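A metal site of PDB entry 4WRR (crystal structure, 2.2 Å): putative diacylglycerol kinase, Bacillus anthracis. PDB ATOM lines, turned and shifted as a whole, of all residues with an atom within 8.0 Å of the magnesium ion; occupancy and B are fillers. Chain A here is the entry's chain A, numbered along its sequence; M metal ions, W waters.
Water W1 lies within hydrogen-bond range of the side-chain carboxylate of Asp 219, the side-chain carboxylate of Asp 223 and the backbone NH of Lys 216.
Water W3 bridges the backbone carbonyl oxygen of Gly 200 and the side-chain carboxylate of Asp 223.
Water W2 bridges OD2 of Asp 127 (2.7 Å) and OD1 of Asn 201 (2.9 Å).
The magnesium ion is bound by water W3, water W2, O of Thr 221, O of Lys 216, OD1 of Asp 219 and water W1.
OD2 of Asp 127 sits at hydrogen-bond distance from N of Asp 219 (3.3 Å).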
ATOM      1  N   ASP A 127       6.194  32.389  -0.529  1.00  0.00           N
ATOM      2  CA  ASP A 127       6.749  32.332  -1.869  1.00  0.00           C
ATOM      3  C   ASP A 127       6.144  31.190  -2.661  1.00  0.00           C
ATOM      4  O   ASP A 127       5.822  30.133  -2.101  1.00  0.00           O
ATOM      5  CB  ASP A 127       8.277  32.122  -1.849  1.00  0.00           C
ATOM      6  CG  ASP A 127       9.025  33.153  -1.004  1.00  0.00           C
ATOM      7  OD1 ASP A 127       8.513  34.294  -0.824  1.00  0.00           O
ATOM      8  OD2 ASP A 127      10.150  32.829  -0.564  1.00  0.00           O
ATOM      9  N   GLY A 200      13.474  22.655  -3.836  1.00  0.00           N
ATOM     10  CA  GLY A 200      12.539  22.684  -2.727  1.00  0.00           C
ATOM     11  C   GLY A 200      12.126  24.092  -2.301  1.00  0.00           C
ATOM     12  O   GLY A 200      12.963  25.029  -2.253  1.00  0.00           O
ATOM     13  N   ASN A 201      10.846  24.224  -1.999  1.00  0.00           N
ATOM     14  CA  ASN A 201      10.220  25.404  -1.422  1.00  0.00           C
ATOM     15  C   ASN A 201       9.468  25.112  -0.114  1.00  0.00           C
ATOM     16  O   ASN A 201       9.406  25.967   0.761  1.00  0.00           O
ATOM     17  CB  ASN A 201       9.226  25.975  -2.425  1.00  0.00           C
ATOM     18  CG  ASN A 201       8.742  27.350  -2.034  1.00  0.00           C
ATOM     19  OD1 ASN A 201       9.552  28.274  -1.903  1.00  0.00           O
ATOM     20  ND2 ASN A 201       7.426  27.484  -1.780  1.00  0.00           N
ATOM     21  N   GLY A 202       8.947  23.898   0.052  1.00  0.00           N
ATOM     22  CA  GLY A 202       8.268  23.493   1.298  1.00  0.00           C
ATOM     23  C   GLY A 202       9.177  23.097   2.429  1.00  0.00           C
ATOM     24  O   GLY A 202      10.301  22.618   2.186  1.00  0.00           O
ATOM     25  N   GLU A 203       8.749  23.338   3.652  1.00  0.00           N
ATOM     26  CA  GLU A 203       9.516  22.996   4.841  1.00  0.00           C
ATOM     27  C   GLU A 203       9.290  21.534   5.259  1.00  0.00           C
ATOM     28  O   GLU A 203      10.023  21.015   6.090  1.00  0.00           O
ATOM     29  CB  GLU A 203       9.254  24.019   5.967  1.00  0.00           C
ATOM     30  CG  GLU A 203       9.642  25.451   5.549  1.00  0.00           C
ATOM     31  CD  GLU A 203       9.268  26.552   6.513  1.00  0.00           C
ATOM     32  OE1 GLU A 203       9.116  27.736   6.072  1.00  0.00           O
ATOM     33  OE2 GLU A 203       9.136  26.303   7.718  1.00  0.00           O
ATOM     34  N   ASN A 214      17.281  23.219   5.827  1.00  0.00           N
ATOM     35  CA  ASN A 214      17.045  24.625   6.054  1.00  0.00           C
ATOM     36  C   ASN A 214      16.233  25.345   4.980  1.00  0.00           C
ATOM     37  O   ASN A 214      16.515  26.508   4.659  1.00  0.00           O
ATOM     38  CB  ASN A 214      18.398  25.338   6.267  1.00  0.00           C
ATOM     39  CG  ASN A 214      19.210  24.682   7.409  1.00  0.00           C
ATOM     40  OD1 ASN A 214      20.259  24.116   7.176  1.00  0.00           O
ATOM     41  ND2 ASN A 214      18.690  24.737   8.625  1.00  0.00           N
ATOM     42  N   VAL A 215      15.268  24.640   4.416  1.00  0.00           N
ATOM     43  CA  VAL A 215      14.303  25.225   3.502  1.00  0.00           C
ATOM     44  C   VAL A 215      13.293  26.098   4.242  1.00  0.00           C
ATOM     45  O   VAL A 215      12.845  25.757   5.327  1.00  0.00           O
ATOM     46  CB  VAL A 215      13.620  24.160   2.702  1.00  0.00           C
ATOM     47  CG1 VAL A 215      12.573  24.786   1.790  1.00  0.00           C
ATOM     48  CG2 VAL A 215      14.642  23.394   1.907  1.00  0.00           C
ATOM     49  N   LYS A 216      13.017  27.284   3.706  1.00  0.00           N
ATOM     50  CA  LYS A 216      11.992  28.156   4.224  1.00  0.00           C
ATOM     51  C   LYS A 216      11.129  28.552   3.048  1.00  0.00           C
ATOM     52  O   LYS A 216      11.653  28.829   1.969  1.00  0.00           O
ATOM     53  CB  LYS A 216      12.579  29.411   4.863  1.00  0.00           C
ATOM     54  CG  LYS A 216      13.473  29.135   6.071  1.00  0.00           C
ATOM     55  CD  LYS A 216      12.634  28.685   7.278  1.00  0.00           C
ATOM     56  CE  LYS A 216      13.510  28.083   8.382  1.00  0.00           C
ATOM     57  NZ  LYS A 216      12.826  28.026   9.713  1.00  0.00           N
ATOM     58  N   CYS A 217       9.805  28.570   3.244  1.00  0.00           N
ATOM     59  CA  CYS A 217       8.876  28.887   2.166  1.00  0.00           C
ATOM     60  C   CYS A 217       8.751  30.419   1.899  1.00  0.00           C
ATOM     61  O   CYS A 217       8.016  30.812   1.054  1.00  0.00           O
ATOM     62  CB  CYS A 217       7.476  28.317   2.459  1.00  0.00           C
ATOM     63  SG  CYS A 217       6.647  29.163   3.846  1.00  0.00           S
ATOM     64  N   ASP A 218       9.435  31.257   2.677  1.00  0.00           N
ATOM     65  CA  ASP A 218       9.264  32.728   2.572  1.00  0.00           C
ATOM     66  C   ASP A 218      10.597  33.510   2.635  1.00  0.00           C
ATOM     67  O   ASP A 218      10.605  34.677   3.008  1.00  0.00           O
ATOM     68  CB  ASP A 218       8.342  33.203   3.691  1.00  0.00           C
ATOM     69  CG  ASP A 218       8.784  32.737   5.075  1.00  0.00           C
ATOM     70  OD1 ASP A 218       9.794  31.983   5.198  1.00  0.00           O
ATOM     71  OD2 ASP A 218       8.088  33.103   6.057  1.00  0.00           O
ATOM     72  N   ASP A 219      11.711  32.865   2.344  1.00  0.00           N
ATOM     73  CA  ASP A 219      13.005  33.546   2.415  1.00  0.00           C
ATOM     74  C   ASP A 219      13.487  34.096   1.072  1.00  0.00           C
ATOM     75  O   ASP A 219      14.593  34.586   0.995  1.00  0.00           O
ATOM     76  CB  ASP A 219      14.080  32.662   3.040  1.00  0.00           C
ATOM     77  CG  ASP A 219      14.451  31.481   2.167  1.00  0.00           C
ATOM     78  OD1 ASP A 219      13.748  31.220   1.145  1.00  0.00           O
ATOM     79  OD2 ASP A 219      15.395  30.757   2.544  1.00  0.00           O
ATOM     80  N   GLY A 220      12.663  34.018   0.030  1.00  0.00           N
ATOM     81  CA  GLY A 220      12.956  34.643  -1.249  1.00  0.00           C
ATOM     82  C   GLY A 220      13.960  33.909  -2.120  1.00  0.00           C
ATOM     83  O   GLY A 220      14.330  34.428  -3.141  1.00  0.00           O
ATOM     84  N   THR A 221      14.409  32.711  -1.726  1.00  0.00           N
ATOM     85  CA  THR A 221      15.231  31.854  -2.570  1.00  0.00           C
ATOM     86  C   THR A 221      14.756  30.413  -2.549  1.00  0.00           C
ATOM     87  O   THR A 221      14.044  29.994  -1.628  1.00  0.00           O
ATOM     88  CB  THR A 221      16.728  31.805  -2.136  1.00  0.00           C
ATOM     89  OG1 THR A 221      16.848  31.319  -0.770  1.00  0.00           O
ATOM     90  CG2 THR A 221      17.343  33.111  -2.217  1.00  0.00           C
ATOM     91  N   LEU A 222      15.130  29.662  -3.570  1.00  0.00           N
ATOM     92  CA  LEU A 222      14.835  28.256  -3.664  1.00  0.00           C
ATOM     93  C   LEU A 222      16.079  27.461  -3.344  1.00  0.00           C
ATOM     94  O   LEU A 222      17.171  27.988  -3.374  1.00  0.00           O
ATOM     95  CB  LEU A 222      14.398  27.924  -5.070  1.00  0.00           C
ATOM     96  CG  LEU A 222      12.988  28.407  -5.405  1.00  0.00           C
ATOM     97  CD1 LEU A 222      12.795  28.314  -6.902  1.00  0.00           C
ATOM     98  CD2 LEU A 222      11.927  27.577  -4.688  1.00  0.00           C
ATOM     99  N   ASP A 223      15.895  26.186  -3.032  1.00  0.00           N
ATOM    100  CA  ASP A 223      16.970  25.307  -2.600  1.00  0.00           C
ATOM    101  C   ASP A 223      17.155  24.198  -3.609  1.00  0.00           C
ATOM    102  O   ASP A 223      16.215  23.466  -3.883  1.00  0.00           O
ATOM    103  CB  ASP A 223      16.664  24.694  -1.231  1.00  0.00           C
ATOM    104  CG  ASP A 223      16.954  25.640  -0.095  1.00  0.00           C
ATOM    105  OD1 ASP A 223      16.165  26.579   0.119  1.00  0.00           O
ATOM    106  OD2 ASP A 223      18.011  25.459   0.577  1.00  0.00           O
ATOM    107  N   LYS A 256      21.468  27.538  -2.470  1.00  0.00           N
ATOM    108  CA  LYS A 256      20.306  28.419  -2.592  1.00  0.00           C
ATOM    109  C   LYS A 256      20.446  29.341  -3.830  1.00  0.00           C
ATOM    110  O   LYS A 256      21.520  29.868  -4.069  1.00  0.00           O
ATOM    111  CB  LYS A 256      20.153  29.246  -1.312  1.00  0.00           C
ATOM    112  CG  LYS A 256      19.564  28.433  -0.144  1.00  0.00           C
ATOM    113  CD  LYS A 256      19.402  29.320   1.095  1.00  0.00           C
ATOM    114  CE  LYS A 256      18.368  28.820   2.116  1.00  0.00           C
ATOM    115  NZ  LYS A 256      18.361  27.350   2.341  1.00  0.00           N
ATOM    116  N   ALA A 257      19.373  29.496  -4.589  1.00  0.00           N
ATOM    117  CA  ALA A 257      19.353  30.361  -5.758  1.00  0.00           C
ATOM    118  C   ALA A 257      17.923  30.815  -6.130  1.00  0.00           C
ATOM    119  O   ALA A 257      16.957  30.137  -5.818  1.00  0.00           O
ATOM    120  CB  ALA A 257      19.978  29.623  -6.919  1.00  0.00           C
ATOM    121  N   LEU A 286      11.196  32.147  -8.794  1.00  0.00           N
ATOM    122  CA  LEU A 286      10.508  32.292  -7.540  1.00  0.00           C
ATOM    123  C   LEU A 286       9.690  33.574  -7.479  1.00  0.00           C
ATOM    124  O   LEU A 286      10.191  34.651  -7.746  1.00  0.00           O
ATOM    125  CB  LEU A 286      11.502  32.280  -6.365  1.00  0.00           C
ATOM    126  CG  LEU A 286      10.820  32.210  -5.018  1.00  0.00           C
ATOM    127  CD1 LEU A 286      10.180  30.846  -4.787  1.00  0.00           C
ATOM    128  CD2 LEU A 286      11.780  32.525  -3.917  1.00  0.00           C
HETATM  129 MG    MG M   1      12.950  29.230   0.173  1.00  0.00          MG
HETATM  130  O   HOH W   1      14.778  28.421   1.567  1.00  0.00           O
HETATM  131  O   HOH W   2      11.239  30.339  -0.738  1.00  0.00           O
HETATM  132  O   HOH W   3      13.458  27.295  -0.787  1.00  0.00           O
